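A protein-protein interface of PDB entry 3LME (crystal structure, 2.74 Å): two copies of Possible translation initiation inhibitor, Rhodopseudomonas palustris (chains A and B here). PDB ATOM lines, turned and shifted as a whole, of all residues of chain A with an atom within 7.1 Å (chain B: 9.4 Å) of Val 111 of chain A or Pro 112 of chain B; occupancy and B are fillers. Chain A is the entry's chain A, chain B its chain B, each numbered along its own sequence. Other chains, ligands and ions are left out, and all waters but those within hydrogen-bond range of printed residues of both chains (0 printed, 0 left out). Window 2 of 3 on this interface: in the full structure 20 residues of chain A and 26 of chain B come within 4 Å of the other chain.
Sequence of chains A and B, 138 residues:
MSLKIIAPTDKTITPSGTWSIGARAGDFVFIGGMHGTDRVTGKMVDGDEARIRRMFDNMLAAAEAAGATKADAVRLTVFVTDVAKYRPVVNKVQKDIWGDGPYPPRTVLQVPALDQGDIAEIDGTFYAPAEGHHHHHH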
ATOM      1  N   PHE A  79     -21.622  -4.166 -35.800  1.00  0.00           N
ATOM      2  CA  PHE A  79     -21.823  -3.335 -34.618  1.00  0.00           C
ATOM      3  C   PHE A  79     -22.198  -1.928 -35.071  1.00  0.00           C
ATOM      4  O   PHE A  79     -21.502  -1.298 -35.867  1.00  0.00           O
ATOM      5  CB  PHE A  79     -20.556  -3.292 -33.772  1.00  0.00           C
ATOM      6  CG  PHE A  79     -19.933  -4.636 -33.547  1.00  0.00           C
ATOM      7  CD1 PHE A  79     -20.266  -5.389 -32.431  1.00  0.00           C
ATOM      8  CD2 PHE A  79     -19.008  -5.149 -34.449  1.00  0.00           C
ATOM      9  CE1 PHE A  79     -19.698  -6.638 -32.213  1.00  0.00           C
ATOM     10  CE2 PHE A  79     -18.411  -6.412 -34.231  1.00  0.00           C
ATOM     11  CZ  PHE A  79     -18.770  -7.150 -33.107  1.00  0.00           C
ATOM     12  N   VAL A  80     -23.323  -1.449 -34.578  1.00  0.00           N
ATOM     13  CA  VAL A  80     -23.771  -0.119 -34.882  1.00  0.00           C
ATOM     14  C   VAL A  80     -24.094   0.643 -33.591  1.00  0.00           C
ATOM     15  O   VAL A  80     -24.072   0.108 -32.478  1.00  0.00           O
ATOM     16  CB  VAL A  80     -25.014  -0.123 -35.818  1.00  0.00           C
ATOM     17  CG1 VAL A  80     -24.808  -1.058 -36.978  1.00  0.00           C
ATOM     18  CG2 VAL A  80     -26.270  -0.498 -35.045  1.00  0.00           C
ATOM     19  N   THR A  81     -24.433   1.905 -33.782  1.00  0.00           N
ATOM     20  CA  THR A  81     -24.496   2.876 -32.736  1.00  0.00           C
ATOM     21  C   THR A  81     -25.935   3.136 -32.309  1.00  0.00           C
ATOM     22  O   THR A  81     -26.181   3.622 -31.183  1.00  0.00           O
ATOM     23  CB  THR A  81     -23.734   4.122 -33.210  1.00  0.00           C
ATOM     24  OG1 THR A  81     -22.545   4.204 -32.434  1.00  0.00           O
ATOM     25  CG2 THR A  81     -24.555   5.441 -33.117  1.00  0.00           C
ATOM     26  N   ASP A  82     -26.866   2.783 -33.206  1.00  0.00           N
ATOM     27  CA  ASP A  82     -28.301   2.920 -32.996  1.00  0.00           C
ATOM     28  C   ASP A  82     -28.969   1.855 -33.863  1.00  0.00           C
ATOM     29  O   ASP A  82     -29.278   2.073 -35.015  1.00  0.00           O
ATOM     30  CB  ASP A  82     -28.750   4.348 -33.363  1.00  0.00           C
ATOM     31  CG  ASP A  82     -30.251   4.617 -33.101  1.00  0.00           C
ATOM     32  OD1 ASP A  82     -31.036   3.694 -32.753  1.00  0.00           O
ATOM     33  OD2 ASP A  82     -30.649   5.790 -33.267  1.00  0.00           O
ATOM     34  N   VAL A  83     -29.180   0.678 -33.305  1.00  0.00           N
ATOM     35  CA  VAL A  83     -29.801  -0.406 -34.053  1.00  0.00           C
ATOM     36  C   VAL A  83     -31.160   0.007 -34.636  1.00  0.00           C
ATOM     37  O   VAL A  83     -31.441  -0.249 -35.794  1.00  0.00           O
ATOM     38  CB  VAL A  83     -29.843  -1.736 -33.220  1.00  0.00           C
ATOM     39  CG1 VAL A  83     -30.893  -1.685 -32.108  1.00  0.00           C
ATOM     40  CG2 VAL A  83     -30.058  -2.932 -34.121  1.00  0.00           C
ATOM     41  N   LEU A 109     -25.643  -5.869 -33.544  1.00  0.00           N
ATOM     42  CA  LEU A 109     -25.818  -5.381 -32.153  1.00  0.00           C
ATOM     43  C   LEU A 109     -25.601  -3.895 -32.035  1.00  0.00           C
ATOM     44  O   LEU A 109     -24.822  -3.324 -32.795  1.00  0.00           O
ATOM     45  CB  LEU A 109     -24.846  -6.054 -31.190  1.00  0.00           C
ATOM     46  CG  LEU A 109     -24.360  -7.419 -31.634  1.00  0.00           C
ATOM     47  CD1 LEU A 109     -22.892  -7.460 -31.397  1.00  0.00           C
ATOM     48  CD2 LEU A 109     -25.077  -8.523 -30.901  1.00  0.00           C
ATOM     49  N   GLN A 110     -26.282  -3.277 -31.074  1.00  0.00           N
ATOM     50  CA  GLN A 110     -25.992  -1.892 -30.716  1.00  0.00           C
ATOM     51  C   GLN A 110     -24.832  -1.858 -29.743  1.00  0.00           C
ATOM     52  O   GLN A 110     -24.645  -2.777 -28.954  1.00  0.00           O
ATOM     53  CB  GLN A 110     -27.206  -1.213 -30.113  1.00  0.00           C
ATOM     54  CG  GLN A 110     -27.112   0.286 -30.059  1.00  0.00           C
ATOM     55  CD  GLN A 110     -28.409   0.904 -29.568  1.00  0.00           C
ATOM     56  OE1 GLN A 110     -29.464   0.746 -30.201  1.00  0.00           O
ATOM     57  NE2 GLN A 110     -28.346   1.594 -28.417  1.00  0.00           N
ATOM     58  N   VAL A 111     -24.064  -0.786 -29.780  1.00  0.00           N
ATOM     59  CA  VAL A 111     -22.849  -0.711 -28.994  1.00  0.00           C
ATOM     60  C   VAL A 111     -22.653   0.784 -28.677  1.00  0.00           C
ATOM     61  O   VAL A 111     -23.192   1.617 -29.386  1.00  0.00           O
ATOM     62  CB  VAL A 111     -21.728  -1.414 -29.796  1.00  0.00           C
ATOM     63  CG1 VAL A 111     -20.707  -0.449 -30.347  1.00  0.00           C
ATOM     64  CG2 VAL A 111     -21.095  -2.499 -28.970  1.00  0.00           C
ATOM     65  N   PRO A 112     -21.956   1.147 -27.587  1.00  0.00           N
ATOM     66  CA  PRO A 112     -21.959   2.604 -27.323  1.00  0.00           C
ATOM     67  C   PRO A 112     -20.942   3.422 -28.128  1.00  0.00           C
ATOM     68  O   PRO A 112     -21.265   4.511 -28.580  1.00  0.00           O
ATOM     69  CB  PRO A 112     -21.647   2.696 -25.815  1.00  0.00           C
ATOM     70  CG  PRO A 112     -21.798   1.289 -25.282  1.00  0.00           C
ATOM     71  CD  PRO A 112     -21.415   0.407 -26.436  1.00  0.00           C
ATOM     72  N   ALA A 113     -19.727   2.918 -28.310  1.00  0.00           N
ATOM     73  CA  ALA A 113     -18.713   3.688 -29.044  1.00  0.00           C
ATOM     74  C   ALA A 113     -17.907   2.822 -30.015  1.00  0.00           C
ATOM     75  O   ALA A 113     -17.711   1.622 -29.769  1.00  0.00           O
ATOM     76  CB  ALA A 113     -17.785   4.441 -28.075  1.00  0.00           C
ATOM     77  N   LEU A 114     -17.450   3.428 -31.118  1.00  0.00           N
ATOM     78  CA  LEU A 114     -16.755   2.671 -32.181  1.00  0.00           C
ATOM     79  C   LEU A 114     -15.395   3.253 -32.509  1.00  0.00           C
ATOM     80  O   LEU A 114     -15.107   4.376 -32.099  1.00  0.00           O
ATOM     81  CB  LEU A 114     -17.621   2.614 -33.456  1.00  0.00           C
ATOM     82  CG  LEU A 114     -18.674   1.521 -33.368  1.00  0.00           C
ATOM     83  CD1 LEU A 114     -19.519   1.476 -34.594  1.00  0.00           C
ATOM     84  CD2 LEU A 114     -18.018   0.180 -33.128  1.00  0.00           C
ATOM     85  N   PHE B  79     -24.569 -12.108 -26.178  1.00  0.00           N
ATOM     86  CA  PHE B  79     -24.797 -10.683 -25.981  1.00  0.00           C
ATOM     87  C   PHE B  79     -26.059 -10.480 -25.176  1.00  0.00           C
ATOM     88  O   PHE B  79     -27.150 -10.857 -25.609  1.00  0.00           O
ATOM     89  CB  PHE B  79     -24.921  -9.985 -27.338  1.00  0.00           C
ATOM     90  CG  PHE B  79     -23.780 -10.275 -28.268  1.00  0.00           C
ATOM     91  CD1 PHE B  79     -22.613  -9.523 -28.209  1.00  0.00           C
ATOM     92  CD2 PHE B  79     -23.861 -11.314 -29.185  1.00  0.00           C
ATOM     93  CE1 PHE B  79     -21.559  -9.783 -29.031  1.00  0.00           C
ATOM     94  CE2 PHE B  79     -22.801 -11.591 -30.025  1.00  0.00           C
ATOM     95  CZ  PHE B  79     -21.649 -10.812 -29.952  1.00  0.00           C
ATOM     96  N   VAL B  80     -25.914  -9.908 -23.992  1.00  0.00           N
ATOM     97  CA  VAL B  80     -27.065  -9.712 -23.118  1.00  0.00           C
ATOM     98  C   VAL B  80     -27.210  -8.255 -22.734  1.00  0.00           C
ATOM     99  O   VAL B  80     -26.245  -7.489 -22.771  1.00  0.00           O
ATOM    100  CB  VAL B  80     -27.025 -10.589 -21.808  1.00  0.00           C
ATOM    101  CG1 VAL B  80     -26.564 -12.011 -22.080  1.00  0.00           C
ATOM    102  CG2 VAL B  80     -26.163  -9.968 -20.782  1.00  0.00           C
ATOM    103  N   THR B  81     -28.428  -7.912 -22.335  1.00  0.00           N
ATOM    104  CA  THR B  81     -28.848  -6.566 -21.966  1.00  0.00           C
ATOM    105  C   THR B  81     -28.456  -6.148 -20.530  1.00  0.00           C
ATOM    106  O   THR B  81     -28.469  -4.950 -20.199  1.00  0.00           O
ATOM    107  CB  THR B  81     -30.369  -6.490 -22.191  1.00  0.00           C
ATOM    108  OG1 THR B  81     -30.613  -6.138 -23.557  1.00  0.00           O
ATOM    109  CG2 THR B  81     -31.086  -5.521 -21.241  1.00  0.00           C
ATOM    110  N   ASP B  82     -28.082  -7.132 -19.696  1.00  0.00           N
ATOM    111  CA  ASP B  82     -27.811  -6.944 -18.252  1.00  0.00           C
ATOM    112  C   ASP B  82     -26.973  -8.143 -17.789  1.00  0.00           C
ATOM    113  O   ASP B  82     -27.524  -9.204 -17.500  1.00  0.00           O
ATOM    114  CB  ASP B  82     -29.155  -6.890 -17.485  1.00  0.00           C
ATOM    115  CG  ASP B  82     -29.035  -6.320 -16.069  1.00  0.00           C
ATOM    116  OD1 ASP B  82     -28.086  -6.657 -15.331  1.00  0.00           O
ATOM    117  OD2 ASP B  82     -29.928  -5.544 -15.668  1.00  0.00           O
ATOM    118  N   VAL B  83     -25.651  -7.999 -17.729  1.00  0.00           N
ATOM    119  CA  VAL B  83     -24.803  -9.147 -17.378  1.00  0.00           C
ATOM    120  C   VAL B  83     -25.115  -9.672 -15.990  1.00  0.00           C
ATOM    121  O   VAL B  83     -25.083 -10.883 -15.754  1.00  0.00           O
ATOM    122  CB  VAL B  83     -23.306  -8.824 -17.331  1.00  0.00           C
ATOM    123  CG1 VAL B  83     -22.508 -10.004 -17.841  1.00  0.00           C
ATOM    124  CG2 VAL B  83     -23.000  -7.587 -18.097  1.00  0.00           C
ATOM    125  N   LEU B 109     -21.344 -10.704 -22.792  1.00  0.00           N
ATOM    126  CA  LEU B 109     -21.130  -9.265 -22.942  1.00  0.00           C
ATOM    127  C   LEU B 109     -22.397  -8.527 -22.706  1.00  0.00           C
ATOM    128  O   LEU B 109     -23.460  -8.951 -23.167  1.00  0.00           O
ATOM    129  CB  LEU B 109     -20.656  -8.937 -24.362  1.00  0.00           C
ATOM    130  CG  LEU B 109     -19.339  -9.656 -24.623  1.00  0.00           C
ATOM    131  CD1 LEU B 109     -19.098  -9.862 -26.074  1.00  0.00           C
ATOM    132  CD2 LEU B 109     -18.192  -8.888 -23.963  1.00  0.00           C
ATOM    133  N   GLN B 110     -22.299  -7.404 -22.005  1.00  0.00           N
ATOM    134  CA  GLN B 110     -23.431  -6.516 -21.951  1.00  0.00           C
ATOM    135  C   GLN B 110     -23.378  -5.606 -23.177  1.00  0.00           C
ATOM    136  O   GLN B 110     -22.322  -5.374 -23.736  1.00  0.00           O
ATOM    137  CB  GLN B 110     -23.500  -5.738 -20.645  1.00  0.00           C
ATOM    138  CG  GLN B 110     -24.904  -5.232 -20.398  1.00  0.00           C
ATOM    139  CD  GLN B 110     -25.065  -4.550 -19.082  1.00  0.00           C
ATOM    140  OE1 GLN B 110     -24.701  -5.091 -18.044  1.00  0.00           O
ATOM    141  NE2 GLN B 110     -25.640  -3.363 -19.101  1.00  0.00           N
ATOM    142  N   VAL B 111     -24.530  -5.095 -23.574  1.00  0.00           N
ATOM    143  CA  VAL B 111     -24.688  -4.447 -24.832  1.00  0.00           C
ATOM    144  C   VAL B 111     -25.984  -3.636 -24.643  1.00  0.00           C
ATOM    145  O   VAL B 111     -26.930  -4.160 -24.066  1.00  0.00           O
ATOM    146  CB  VAL B 111     -24.723  -5.573 -25.929  1.00  0.00           C
ATOM    147  CG1 VAL B 111     -26.113  -5.807 -26.534  1.00  0.00           C
ATOM    148  CG2 VAL B 111     -23.650  -5.356 -26.972  1.00  0.00           C
ATOM    149  N   PRO B 112     -26.027  -2.348 -25.084  1.00  0.00           N
ATOM    150  CA  PRO B 112     -27.163  -1.489 -24.741  1.00  0.00           C
ATOM    151  C   PRO B 112     -28.500  -1.912 -25.339  1.00  0.00           C
ATOM    152  O   PRO B 112     -29.550  -1.631 -24.745  1.00  0.00           O
ATOM    153  CB  PRO B 112     -26.751  -0.130 -25.288  1.00  0.00           C
ATOM    154  CG  PRO B 112     -25.809  -0.438 -26.359  1.00  0.00           C
ATOM    155  CD  PRO B 112     -25.034  -1.605 -25.876  1.00  0.00           C
ATOM    156  N   ALA B 113     -28.476  -2.568 -26.495  1.00  0.00           N
ATOM    157  CA  ALA B 113     -29.715  -3.038 -27.128  1.00  0.00           C
ATOM    158  C   ALA B 113     -29.461  -4.085 -28.197  1.00  0.00           C
ATOM    159  O   ALA B 113     -28.390  -4.122 -28.812  1.00  0.00           O
ATOM    160  CB  ALA B 113     -30.536  -1.866 -27.701  1.00  0.00           C
ATOM    161  N   LEU B 114     -30.453  -4.948 -28.385  1.00  0.00           N
ATOM    162  CA  LEU B 114     -30.450  -5.944 -29.445  1.00  0.00           C
ATOM    163  C   LEU B 114     -31.680  -5.634 -30.256  1.00  0.00           C
ATOM    164  O   LEU B 114     -32.530  -4.868 -29.813  1.00  0.00           O
ATOM    165  CB  LEU B 114     -30.537  -7.359 -28.866  1.00  0.00           C
ATOM    166  CG  LEU B 114     -29.408  -7.731 -27.905  1.00  0.00           C
ATOM    167  CD1 LEU B 114     -29.882  -8.749 -26.924  1.00  0.00           C
ATOM    168  CD2 LEU B 114     -28.182  -8.212 -28.644  1.00  0.00           C
ATOM    169  N   ASP B 115     -31.789  -6.201 -31.448  1.00  0.00           N
ATOM    170  CA  ASP B 115     -32.932  -5.861 -32.272  1.00  0.00           C
ATOM    171  C   ASP B 115     -34.211  -6.440 -31.642  1.00  0.00           C
ATOM    172  O   ASP B 115     -34.155  -7.448 -30.893  1.00  0.00           O
ATOM    173  CB  ASP B 115     -32.745  -6.320 -33.733  1.00  0.00           C
ATOM    174  CG  ASP B 115     -33.600  -5.490 -34.731  1.00  0.00           C
ATOM    175  OD1 ASP B 115     -33.204  -4.336 -35.073  1.00  0.00           O
ATOM    176  OD2 ASP B 115     -34.663  -6.004 -35.175  1.00  0.00           O
ATOM    177  N   GLY B 117     -35.789  -5.391 -29.369  1.00  0.00           N
ATOM    178  CA  GLY B 117     -35.750  -5.090 -27.936  1.00  0.00           C
ATOM    179  C   GLY B 117     -35.487  -6.284 -27.021  1.00  0.00           C
ATOM    180  O   GLY B 117     -35.652  -6.181 -25.797  1.00  0.00           O
ATOM    181  N   ASP B 118     -35.063  -7.413 -27.597  1.00  0.00           N
ATOM    182  CA  ASP B 118     -34.771  -8.603 -26.814  1.00  0.00           C
ATOM    183  C   ASP B 118     -33.635  -8.383 -25.799  1.00  0.00           C
ATOM    184  O   ASP B 118     -32.824  -7.471 -25.952  1.00  0.00           O
ATOM    185  CB  ASP B 118     -34.458  -9.791 -27.726  1.00  0.00           C
ATOM    186  CG  ASP B 118     -34.772 -11.138 -27.073  1.00  0.00           C
ATOM    187  OD1 ASP B 118     -34.768 -11.256 -25.831  1.00  0.00           O
ATOM    188  OD2 ASP B 118     -35.036 -12.105 -27.809  1.00  0.00           O
ATOM    189  N   ILE B 119     -33.596  -9.256 -24.783  1.00  0.00           N
ATOM    190  CA  ILE B 119     -32.632  -9.261 -23.670  1.00  0.00           C
ATOM    191  C   ILE B 119     -31.323 -10.048 -23.924  1.00  0.00           C
ATOM    192  O   ILE B 119     -30.298  -9.818 -23.252  1.00  0.00           O
ATOM    193  CB  ILE B 119     -33.296  -9.855 -22.414  1.00  0.00           C
ATOM    194  CG1 ILE B 119     -33.345 -11.392 -22.537  1.00  0.00           C
ATOM    195  CG2 ILE B 119     -34.683  -9.188 -22.186  1.00  0.00           C
ATOM    196  CD1 ILE B 119     -34.059 -12.148 -21.405  1.00  0.00           C
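The backbone NH (N) of Gln 110 of chain A is in hydrogen-bond range of the backbone carbonyl oxygen (O) of Ala 113 of chain B, 3.2 Å away.
The backbone NH (N) of Val 80 of chain A is in hydrogen-bond range of the backbone carbonyl oxygen (O) of Leu 109 of chain A, at 3.0 Å.
The backbone carbonyl oxygen (O) of Val 80 of chain A is in hydrogen-bond range of the backbone NH (N) of Val 111 of chain A, at 2.8 Å.
OE1 of Gln 110 of chain A sits at hydrogen-bond distance from N of Val 83 of chain A (3.1 Å).
The backbone NH (N) of Val 111 of chain B is in hydrogen-bond range of the backbone carbonyl oxygen (O) of Val 80 of chain B, at 3.1 Å.
Val 83 of chain A touches Asp 115 of chain B (CG2 to OD1, 3.6 Å).
Leu 109 of chain A touches Phe 79 of chain B.
Leu 109 of chain A touches Leu 114 of chain B (CD2 to CD2, 3.9 Å).
Gln 110 of chain A touches Val 111 of chain B.
O of Gln 110 of chain A touches CD of Pro 112 of chain B, 3.3 Å away.
Val 111 of chain A touches Pro 112 of chain B.
Val 80 of chain A touches none of the printed residues of chain B.
Val 111 of chain A touches just one residue of chain B: Pro 112.
No residue of chain B comes within 4 Å of Pro 112 of chain A.
Ala 113 of chain A touches none of the printed residues of chain B.
Printed residues of chain A within 4 Å of Phe 79 of chain B: Leu 109 (3.4 Å).
Printed residues of chain A within 4 Å of Val 111 of chain B: Gln 110.
Pro 112 of chain B touches just these residues of chain A: Gln 110 and Val 111.
Printed residues of chain A within 4 Å of Asp 115 of chain B: Val 83 (3.6 Å).
The nearest residue of chain A that does not touch Pro 112 of chain B is Pro 112 of chain A (4.2 Å).
Of the 15 printed residues of chain B, 6 touch a printed residue of chain A.
Printed residues of chain B that touch a printed residue of chain A: Phe 79, Val 111, Pro 112, Ala 113, Leu 114 and Asp 115.
Of the 11 printed residues of chain A, 4 touch a printed residue of chain B.
Printed residues of chain A that touch a printed residue of chain B: Val 83, Leu 109, Gln 110 and Val 111.
Hydrophobic or aromatic side chains of chain A that line the printed part of chain B: Val 83 and Leu 109.
Leu 109 of chain A touches Leu 114 of chain B, but with the chains exchanged Leu 114 of chain A does not touch Leu 109 of chain B (12.3 Å).
Gln 110 of chain A touches Pro 112 of chain B, but with the chains exchanged Pro 112 of chain A does not touch Gln 110 of chain B (6.4 Å).
Gln 110 of chain A touches Ala 113 of chain B, but with the chains exchanged Ala 113 of chain A does not touch Gln 110 of chain B (9.8 Å).
Val 111 of chain A touches Pro 112 of chain B, but with the chains exchanged Pro 112 of chain A does not touch Val 111 of chain B (6.1 Å).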
